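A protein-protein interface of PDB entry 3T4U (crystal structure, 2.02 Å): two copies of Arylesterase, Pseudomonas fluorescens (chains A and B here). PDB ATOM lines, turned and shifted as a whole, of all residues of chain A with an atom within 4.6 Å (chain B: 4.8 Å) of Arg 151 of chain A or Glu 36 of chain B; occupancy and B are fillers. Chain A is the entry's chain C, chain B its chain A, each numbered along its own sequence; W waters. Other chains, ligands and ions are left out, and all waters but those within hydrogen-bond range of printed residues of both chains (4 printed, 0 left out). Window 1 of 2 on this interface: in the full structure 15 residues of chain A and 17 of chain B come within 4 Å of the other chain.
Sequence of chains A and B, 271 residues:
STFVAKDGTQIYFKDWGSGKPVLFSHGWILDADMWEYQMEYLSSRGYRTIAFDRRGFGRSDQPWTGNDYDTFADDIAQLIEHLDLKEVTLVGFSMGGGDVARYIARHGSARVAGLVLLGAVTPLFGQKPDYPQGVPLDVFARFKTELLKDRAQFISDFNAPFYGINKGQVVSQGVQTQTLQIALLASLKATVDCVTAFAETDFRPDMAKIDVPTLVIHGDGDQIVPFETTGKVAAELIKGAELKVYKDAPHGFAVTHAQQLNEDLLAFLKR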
ATOM      1  N   GLU A 146     -23.311 -22.332  -3.079  1.00  0.00           N
ATOM      2  CA  GLU A 146     -24.528 -21.899  -2.404  1.00  0.00           C
ATOM      3  C   GLU A 146     -24.742 -20.373  -2.531  1.00  0.00           C
ATOM      4  O   GLU A 146     -25.860 -19.940  -2.763  1.00  0.00           O
ATOM      5  CB  GLU A 146     -24.520 -22.331  -0.954  1.00  0.00           C
ATOM      6  CG  GLU A 146     -24.481 -23.858  -0.795  1.00  0.00           C
ATOM      7  CD  GLU A 146     -24.329 -24.291   0.647  1.00  0.00           C
ATOM      8  OE1 GLU A 146     -23.917 -23.459   1.496  1.00  0.00           O
ATOM      9  OE2 GLU A 146     -24.633 -25.469   0.943  1.00  0.00           O
ATOM     10  N   LEU A 147     -23.668 -19.581  -2.420  1.00  0.00           N
ATOM     11  CA  LEU A 147     -23.775 -18.116  -2.632  1.00  0.00           C
ATOM     12  C   LEU A 147     -24.333 -17.760  -4.011  1.00  0.00           C
ATOM     13  O   LEU A 147     -25.140 -16.847  -4.132  1.00  0.00           O
ATOM     14  CB  LEU A 147     -22.414 -17.446  -2.451  1.00  0.00           C
ATOM     15  CG  LEU A 147     -21.975 -17.430  -0.990  1.00  0.00           C
ATOM     16  CD1 LEU A 147     -20.474 -17.179  -0.937  1.00  0.00           C
ATOM     17  CD2 LEU A 147     -22.769 -16.396  -0.128  1.00  0.00           C
ATOM     18  N   LYS A 149     -26.322 -19.464  -5.849  1.00  0.00           N
ATOM     19  CA  LYS A 149     -27.743 -19.833  -5.957  1.00  0.00           C
ATOM     20  C   LYS A 149     -28.642 -18.892  -5.163  1.00  0.00           C
ATOM     21  O   LYS A 149     -29.667 -18.421  -5.673  1.00  0.00           O
ATOM     22  CB  LYS A 149     -27.969 -21.252  -5.425  1.00  0.00           C
ATOM     23  CG  LYS A 149     -27.561 -22.334  -6.394  1.00  0.00           C
ATOM     24  CD  LYS A 149     -27.663 -23.709  -5.739  1.00  0.00           C
ATOM     25  CE  LYS A 149     -26.877 -24.721  -6.554  1.00  0.00           C
ATOM     26  NZ  LYS A 149     -26.984 -26.051  -5.918  1.00  0.00           N
ATOM     27  N   ASP A 150     -28.260 -18.634  -3.908  1.00  0.00           N
ATOM     28  CA  ASP A 150     -29.119 -17.889  -2.966  1.00  0.00           C
ATOM     29  C   ASP A 150     -28.275 -17.377  -1.800  1.00  0.00           C
ATOM     30  O   ASP A 150     -28.191 -18.011  -0.736  1.00  0.00           O
ATOM     31  CB  ASP A 150     -30.281 -18.772  -2.452  1.00  0.00           C
ATOM     32  CG  ASP A 150     -31.269 -18.006  -1.532  1.00  0.00           C
ATOM     33  OD1 ASP A 150     -30.993 -16.838  -1.159  1.00  0.00           O
ATOM     34  OD2 ASP A 150     -32.326 -18.592  -1.159  1.00  0.00           O
ATOM     35  N   ARG A 151     -27.651 -16.221  -1.996  1.00  0.00           N
ATOM     36  CA  ARG A 151     -26.768 -15.681  -0.961  1.00  0.00           C
ATOM     37  C   ARG A 151     -27.491 -15.259   0.319  1.00  0.00           C
ATOM     38  O   ARG A 151     -26.937 -15.385   1.416  1.00  0.00           O
ATOM     39  CB  ARG A 151     -25.893 -14.557  -1.513  1.00  0.00           C
ATOM     40  CG  ARG A 151     -26.505 -13.195  -1.501  1.00  0.00           C
ATOM     41  CD  ARG A 151     -25.460 -12.118  -1.927  1.00  0.00           C
ATOM     42  NE  ARG A 151     -26.154 -10.941  -2.435  1.00  0.00           N
ATOM     43  CZ  ARG A 151     -26.142  -9.728  -1.882  1.00  0.00           C
ATOM     44  NH1 ARG A 151     -26.845  -8.753  -2.460  1.00  0.00           N
ATOM     45  NH2 ARG A 151     -25.474  -9.478  -0.747  1.00  0.00           N
ATOM     46  N   ALA A 152     -28.706 -14.752   0.170  1.00  0.00           N
ATOM     47  CA  ALA A 152     -29.531 -14.284   1.288  1.00  0.00           C
ATOM     48  C   ALA A 152     -29.814 -15.392   2.269  1.00  0.00           C
ATOM     49  O   ALA A 152     -29.654 -15.200   3.476  1.00  0.00           O
ATOM     50  CB  ALA A 152     -30.907 -13.706   0.778  1.00  0.00           C
ATOM     51  N   GLN A 153     -30.232 -16.554   1.763  1.00  0.00           N
ATOM     52  CA  GLN A 153     -30.485 -17.694   2.667  1.00  0.00           C
ATOM     53  C   GLN A 153     -29.158 -18.276   3.208  1.00  0.00           C
ATOM     54  O   GLN A 153     -29.093 -18.721   4.363  1.00  0.00           O
ATOM     55  CB  GLN A 153     -31.334 -18.798   2.016  1.00  0.00           C
ATOM     56  CG  GLN A 153     -31.895 -19.837   3.075  1.00  0.00           C
ATOM     57  CD  GLN A 153     -32.743 -19.208   4.181  1.00  0.00           C
ATOM     58  OE1 GLN A 153     -33.524 -18.291   3.930  1.00  0.00           O
ATOM     59  NE2 GLN A 153     -32.626 -19.732   5.412  1.00  0.00           N
ATOM     60  N   PHE A 154     -28.109 -18.263   2.382  1.00  0.00           N
ATOM     61  CA  PHE A 154     -26.762 -18.611   2.858  1.00  0.00           C
ATOM     62  C   PHE A 154     -26.355 -17.783   4.104  1.00  0.00           C
ATOM     63  O   PHE A 154     -25.963 -18.347   5.103  1.00  0.00           O
ATOM     64  CB  PHE A 154     -25.686 -18.467   1.769  1.00  0.00           C
ATOM     65  CG  PHE A 154     -24.293 -18.859   2.251  1.00  0.00           C
ATOM     66  CD1 PHE A 154     -23.813 -20.145   2.017  1.00  0.00           C
ATOM     67  CD2 PHE A 154     -23.510 -17.961   2.994  1.00  0.00           C
ATOM     68  CE1 PHE A 154     -22.547 -20.526   2.501  1.00  0.00           C
ATOM     69  CE2 PHE A 154     -22.240 -18.318   3.475  1.00  0.00           C
ATOM     70  CZ  PHE A 154     -21.752 -19.592   3.217  1.00  0.00           C
ATOM     71  N   ILE A 155     -26.440 -16.453   4.016  1.00  0.00           N
ATOM     72  CA  ILE A 155     -26.158 -15.559   5.155  1.00  0.00           C
ATOM     73  C   ILE A 155     -27.026 -15.863   6.376  1.00  0.00           C
ATOM     74  O   ILE A 155     -26.536 -15.866   7.517  1.00  0.00           O
ATOM     75  CB  ILE A 155     -26.340 -14.070   4.766  1.00  0.00           C
ATOM     76  CG1 ILE A 155     -25.348 -13.686   3.648  1.00  0.00           C
ATOM     77  CG2 ILE A 155     -26.124 -13.142   5.993  1.00  0.00           C
ATOM     78  CD1 ILE A 155     -25.856 -12.506   2.780  1.00  0.00           C
ATOM     79  N   ALA A 183     -25.241  -7.687   5.697  1.00  0.00           N
ATOM     80  CA  ALA A 183     -24.659  -8.623   4.735  1.00  0.00           C
ATOM     81  C   ALA A 183     -25.292  -8.454   3.355  1.00  0.00           C
ATOM     82  O   ALA A 183     -24.617  -8.577   2.306  1.00  0.00           O
ATOM     83  CB  ALA A 183     -24.846 -10.057   5.244  1.00  0.00           C
ATOM     84  N   LEU A 184     -26.586  -8.130   3.353  1.00  0.00           N
ATOM     85  CA  LEU A 184     -27.321  -7.931   2.076  1.00  0.00           C
ATOM     86  C   LEU A 184     -26.916  -6.639   1.359  1.00  0.00           C
ATOM     87  O   LEU A 184     -27.113  -6.519   0.138  1.00  0.00           O
ATOM     88  CB  LEU A 184     -28.837  -7.977   2.283  1.00  0.00           C
ATOM     89  CG  LEU A 184     -29.335  -9.386   2.682  1.00  0.00           C
ATOM     90  CD1 LEU A 184     -30.798  -9.291   3.187  1.00  0.00           C
ATOM     91  CD2 LEU A 184     -29.205 -10.396   1.538  1.00  0.00           C
ATOM     92  N   ALA A 186     -23.888  -5.930   0.754  1.00  0.00           N
ATOM     93  CA  ALA A 186     -22.698  -6.280  -0.032  1.00  0.00           C
ATOM     94  C   ALA A 186     -23.007  -6.710  -1.442  1.00  0.00           C
ATOM     95  O   ALA A 186     -24.120  -7.159  -1.754  1.00  0.00           O
ATOM     96  CB  ALA A 186     -21.862  -7.403   0.672  1.00  0.00           C
ATOM     97  N   LEU A 188     -22.756  -9.281  -4.473  1.00  0.00           N
ATOM     98  CA  LEU A 188     -22.632 -10.738  -4.679  1.00  0.00           C
ATOM     99  C   LEU A 188     -21.227 -11.071  -5.138  1.00  0.00           C
ATOM    100  O   LEU A 188     -20.613 -12.034  -4.667  1.00  0.00           O
ATOM    101  CB  LEU A 188     -23.622 -11.250  -5.735  1.00  0.00           C
ATOM    102  CG  LEU A 188     -23.402 -12.679  -6.228  1.00  0.00           C
ATOM    103  CD1 LEU A 188     -23.609 -13.712  -5.070  1.00  0.00           C
ATOM    104  CD2 LEU A 188     -24.375 -12.994  -7.373  1.00  0.00           C
ATOM    105  N   TRP B  16     -19.836  -3.448 -14.301  1.00  0.00           N
ATOM    106  CA  TRP B  16     -18.996  -4.587 -13.988  1.00  0.00           C
ATOM    107  C   TRP B  16     -18.465  -5.223 -15.281  1.00  0.00           C
ATOM    108  O   TRP B  16     -19.200  -5.343 -16.257  1.00  0.00           O
ATOM    109  CB  TRP B  16     -19.841  -5.651 -13.282  1.00  0.00           C
ATOM    110  CG  TRP B  16     -20.176  -5.403 -11.847  1.00  0.00           C
ATOM    111  CD1 TRP B  16     -19.771  -4.358 -11.050  1.00  0.00           C
ATOM    112  CD2 TRP B  16     -20.951  -6.265 -11.020  1.00  0.00           C
ATOM    113  NE1 TRP B  16     -20.268  -4.525  -9.768  1.00  0.00           N
ATOM    114  CE2 TRP B  16     -20.987  -5.691  -9.729  1.00  0.00           C
ATOM    115  CE3 TRP B  16     -21.614  -7.481 -11.244  1.00  0.00           C
ATOM    116  CZ2 TRP B  16     -21.684  -6.286  -8.653  1.00  0.00           C
ATOM    117  CZ3 TRP B  16     -22.322  -8.069 -10.186  1.00  0.00           C
ATOM    118  CH2 TRP B  16     -22.323  -7.473  -8.893  1.00  0.00           C
ATOM    119  N   ALA B  32     -31.264  -2.366  -8.560  1.00  0.00           N
ATOM    120  CA  ALA B  32     -30.274  -3.075  -9.378  1.00  0.00           C
ATOM    121  C   ALA B  32     -29.841  -4.440  -8.831  1.00  0.00           C
ATOM    122  O   ALA B  32     -29.338  -5.268  -9.604  1.00  0.00           O
ATOM    123  CB  ALA B  32     -29.016  -2.199  -9.624  1.00  0.00           C
ATOM    124  N   ASP B  33     -29.995  -4.672  -7.519  1.00  0.00           N
ATOM    125  CA  ASP B  33     -29.526  -5.949  -6.922  1.00  0.00           C
ATOM    126  C   ASP B  33     -30.354  -7.108  -7.446  1.00  0.00           C
ATOM    127  O   ASP B  33     -29.910  -8.256  -7.365  1.00  0.00           O
ATOM    128  CB  ASP B  33     -29.538  -5.960  -5.371  1.00  0.00           C
ATOM    129  CG  ASP B  33     -28.516  -5.032  -4.758  1.00  0.00           C
ATOM    130  OD1 ASP B  33     -27.736  -4.370  -5.504  1.00  0.00           O
ATOM    131  OD2 ASP B  33     -28.511  -4.931  -3.504  1.00  0.00           O
ATOM    132  N   MET B  34     -31.551  -6.840  -7.983  1.00  0.00           N
ATOM    133  CA  MET B  34     -32.373  -7.938  -8.535  1.00  0.00           C
ATOM    134  C   MET B  34     -31.616  -8.687  -9.646  1.00  0.00           C
ATOM    135  O   MET B  34     -31.907  -9.851  -9.919  1.00  0.00           O
ATOM    136  CB  MET B  34     -33.763  -7.468  -9.032  1.00  0.00           C
ATOM    137  CG  MET B  34     -33.754  -6.703 -10.406  1.00  0.00           C
ATOM    138  SD  MET B  34     -35.284  -6.894 -11.321  1.00  0.00           S
ATOM    139  CE  MET B  34     -34.944  -8.461 -12.173  1.00  0.00           C
ATOM    140  N   TRP B  35     -30.643  -8.006 -10.250  1.00  0.00           N
ATOM    141  CA  TRP B  35     -29.872  -8.544 -11.372  1.00  0.00           C
ATOM    142  C   TRP B  35     -28.528  -9.178 -11.010  1.00  0.00           C
ATOM    143  O   TRP B  35     -27.820  -9.658 -11.917  1.00  0.00           O
ATOM    144  CB  TRP B  35     -29.578  -7.415 -12.359  1.00  0.00           C
ATOM    145  CG  TRP B  35     -30.778  -6.762 -12.965  1.00  0.00           C
ATOM    146  CD1 TRP B  35     -31.191  -5.465 -12.786  1.00  0.00           C
ATOM    147  CD2 TRP B  35     -31.693  -7.359 -13.886  1.00  0.00           C
ATOM    148  NE1 TRP B  35     -32.313  -5.225 -13.554  1.00  0.00           N
ATOM    149  CE2 TRP B  35     -32.633  -6.376 -14.239  1.00  0.00           C
ATOM    150  CE3 TRP B  35     -31.793  -8.638 -14.470  1.00  0.00           C
ATOM    151  CZ2 TRP B  35     -33.673  -6.630 -15.141  1.00  0.00           C
ATOM    152  CZ3 TRP B  35     -32.821  -8.885 -15.376  1.00  0.00           C
ATOM    153  CH2 TRP B  35     -33.753  -7.891 -15.691  1.00  0.00           C
ATOM    154  N   GLU B  36     -28.160  -9.185  -9.720  1.00  0.00           N
ATOM    155  CA  GLU B  36     -26.768  -9.548  -9.323  1.00  0.00           C
ATOM    156  C   GLU B  36     -26.277 -10.878  -9.892  1.00  0.00           C
ATOM    157  O   GLU B  36     -25.107 -11.002 -10.274  1.00  0.00           O
ATOM    158  CB  GLU B  36     -26.577  -9.539  -7.790  1.00  0.00           C
ATOM    159  CG  GLU B  36     -27.585 -10.438  -6.998  1.00  0.00           C
ATOM    160  CD  GLU B  36     -27.757  -9.997  -5.529  1.00  0.00           C
ATOM    161  OE1 GLU B  36     -27.091  -9.042  -5.076  1.00  0.00           O
ATOM    162  OE2 GLU B  36     -28.574 -10.613  -4.814  1.00  0.00           O
ATOM    163  N   TYR B  37     -27.161 -11.873  -9.909  1.00  0.00           N
ATOM    164  CA  TYR B  37     -26.802 -13.195 -10.440  1.00  0.00           C
ATOM    165  C   TYR B  37     -26.622 -13.195 -11.961  1.00  0.00           C
ATOM    166  O   TYR B  37     -25.726 -13.863 -12.468  1.00  0.00           O
ATOM    167  CB  TYR B  37     -27.818 -14.273 -10.009  1.00  0.00           C
ATOM    168  CG  TYR B  37     -27.882 -14.443  -8.514  1.00  0.00           C
ATOM    169  CD1 TYR B  37     -26.973 -15.281  -7.830  1.00  0.00           C
ATOM    170  CD2 TYR B  37     -28.840 -13.752  -7.765  1.00  0.00           C
ATOM    171  CE1 TYR B  37     -27.023 -15.408  -6.423  1.00  0.00           C
ATOM    172  CE2 TYR B  37     -28.907 -13.879  -6.381  1.00  0.00           C
ATOM    173  CZ  TYR B  37     -27.999 -14.717  -5.717  1.00  0.00           C
ATOM    174  OH  TYR B  37     -28.075 -14.852  -4.354  1.00  0.00           O
ATOM    175  N   GLN B  38     -27.469 -12.471 -12.699  1.00  0.00           N
ATOM    176  CA  GLN B  38     -27.300 -12.400 -14.159  1.00  0.00           C
ATOM    177  C   GLN B  38     -26.036 -11.630 -14.520  1.00  0.00           C
ATOM    178  O   GLN B  38     -25.287 -12.028 -15.445  1.00  0.00           O
ATOM    179  CB  GLN B  38     -28.528 -11.773 -14.835  1.00  0.00           C
ATOM    180  CG  GLN B  38     -29.703 -12.723 -14.949  1.00  0.00           C
ATOM    181  CD  GLN B  38     -30.404 -12.949 -13.614  1.00  0.00           C
ATOM    182  OE1 GLN B  38     -30.768 -11.989 -12.932  1.00  0.00           O
ATOM    183  NE2 GLN B  38     -30.583 -14.214 -13.225  1.00  0.00           N
ATOM    184  N   MET B  39     -25.771 -10.565 -13.762  1.00  0.00           N
ATOM    185  CA  MET B  39     -24.555  -9.740 -13.943  1.00  0.00           C
ATOM    186  C   MET B  39     -23.275 -10.530 -13.685  1.00  0.00           C
ATOM    187  O   MET B  39     -22.339 -10.482 -14.498  1.00  0.00           O
ATOM    188  CB  MET B  39     -24.581  -8.498 -13.040  1.00  0.00           C
ATOM    189  CG  MET B  39     -25.661  -7.506 -13.463  1.00  0.00           C
ATOM    190  SD  MET B  39     -25.683  -6.053 -12.431  1.00  0.00           S
ATOM    191  CE  MET B  39     -24.172  -5.180 -12.927  1.00  0.00           C
ATOM    192  N   GLU B  40     -23.230 -11.239 -12.553  1.00  0.00           N
ATOM    193  CA  GLU B  40     -22.077 -12.069 -12.244  1.00  0.00           C
ATOM    194  C   GLU B  40     -21.907 -13.147 -13.311  1.00  0.00           C
ATOM    195  O   GLU B  40     -20.805 -13.387 -13.772  1.00  0.00           O
ATOM    196  CB  GLU B  40     -22.197 -12.703 -10.858  1.00  0.00           C
ATOM    197  CG  GLU B  40     -20.935 -13.453 -10.410  1.00  0.00           C
ATOM    198  CD  GLU B  40     -20.803 -14.894 -10.972  1.00  0.00           C
ATOM    199  OE1 GLU B  40     -19.686 -15.421 -10.922  1.00  0.00           O
ATOM    200  OE2 GLU B  40     -21.782 -15.498 -11.447  1.00  0.00           O
ATOM    201  N   GLN B 178     -34.720 -10.086   1.690  1.00  0.00           N
ATOM    202  CA  GLN B 178     -33.902  -9.175   0.861  1.00  0.00           C
ATOM    203  C   GLN B 178     -34.805  -8.332  -0.028  1.00  0.00           C
ATOM    204  O   GLN B 178     -34.527  -7.159  -0.261  1.00  0.00           O
ATOM    205  CB  GLN B 178     -32.929  -9.948  -0.039  1.00  0.00           C
ATOM    206  CG  GLN B 178     -31.992  -8.998  -0.860  1.00  0.00           C
ATOM    207  CD  GLN B 178     -31.087  -9.741  -1.820  1.00  0.00           C
ATOM    208  OE1 GLN B 178     -31.294 -10.919  -2.084  1.00  0.00           O
ATOM    209  NE2 GLN B 178     -30.034  -9.065  -2.301  1.00  0.00           N
HETATM  210  O   HOH W   1     -24.896  -7.533  -5.575  1.00  0.00           O
HETATM  211  O   HOH W   2     -29.391  -6.349  -1.319  1.00  0.00           O
HETATM  212  O   HOH W   3     -25.652  -5.443  -3.363  1.00  0.00           O
HETATM  213  O   HOH W   4     -30.175 -14.257  -2.740  1.00  0.00           O
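The side-chain carboxylate (OE1) of Glu 36 of chain B is in salt-bridge range of the guanidinium group (NH1) of Arg 151 of chain A, 2.6 Å away. The side-chain hydroxyl of Tyr 37 of chain B sits at hydrogen-bond distance from the backbone NH of Arg 151 of chain A, 2.8 Å away. NE2 of Gln 178 of chain B lies close to NH1 of Arg 151 of chain A.
Water W2 lies within hydrogen-bond range of the backbone carbonyl oxygen (O) of Leu 184 of chain A (2.7 Å), the side-chain carboxylate (OD2) of Asp 33 of chain B (2.7 Å) and the side-chain amide nitrogen (NE2) of Gln 178 of chain B (3.0 Å). Water W1 lies within hydrogen-bond range of OE1 of Glu 36 of chain B (2.7 Å) and N of Leu 188 of chain A (3.0 Å). Water W4 lies within hydrogen-bond range of OH of Tyr 37 of chain B, OD1 of Asp 150 of chain A, N of Arg 151 of chain A and N of Ala 152 of chain A. Water W3 bridges O of Ala 186 of chain A and OD2 of Asp 33 of chain B.
OE2 of Glu 36 of chain B sits at hydrogen-bond distance from NE2 of Gln 178 of chain B. OD1 of Asp 150 of chain A lies close to N of Ala 152 of chain A (3.4 Å). OD1 of Asp 150 of chain A lies within hydrogen-bond range of N of Gln 153 of chain A, at 3.0 Å. The backbone carbonyl oxygen (O) of Ala 183 of chain A sits at hydrogen-bond distance from the guanidinium group (NH2) of Arg 151 of chain A, 3.3 Å away. O of Leu 184 of chain A is in hydrogen-bond range of NH1 of Arg 151 of chain A (3.4 Å). NH2 of Arg 151 of chain A is in hydrogen-bond range of O of Ala 186 of chain A (2.9 Å).
Of the printed residues of chain B, Asp 150 of chain A touches Tyr 37 (3.5 Å). Arg 151 of chain A touches just these residues of chain B: Glu 36 (2.6 Å), Tyr 37 (2.8 Å) and Gln 178 (3.2 Å). Of the printed residues of chain B, Leu 184 of chain A touches Gln 178. Glu 36 of chain B touches just these residues of chain A: Arg 151 and Leu 188. Printed residues of chain A within 4 Å of Tyr 37 of chain B: Leu 147 (3.3 Å), Asp 150 (3.5 Å), Arg 151 (2.8 Å) and Leu 188 (3.5 Å).
Among the printed residues, pairs that only touch across the chains: Leu 147 of chain A with Tyr 37 of chain B (3.3 Å), Leu 188 of chain A with Tyr 37 of chain B (3.5 Å), Asp 150 of chain A with Tyr 37 of chain B (3.5 Å), Leu 188 of chain A with Glu 36 of chain B (3.6 Å) and Leu 184 of chain A with Gln 178 of chain B (3.9 Å).
No position is printed for both chains. Of the 8 pairs that touch across the chains among the printed residues, none has its exchanged pair printed and touching as well.
Hydrophobic or aromatic side chains of chain B that line the printed part of chain A: Tyr 37. Along chain B the printed residues that touch a printed residue of chain A span positions 36 to 178. Of the 13 printed residues of chain A, 5 touch a printed residue of chain B. Hydrophobic or aromatic side chains of chain A that line the printed part of chain B: Leu 184 and Leu 188. Among the printed residues, Asp or Glu carboxylates within 4 Å of a Lys or Arg side-chain nitrogen of the other chain: Arg 151 of chain A with Glu 36 of chain B (2.6 Å).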
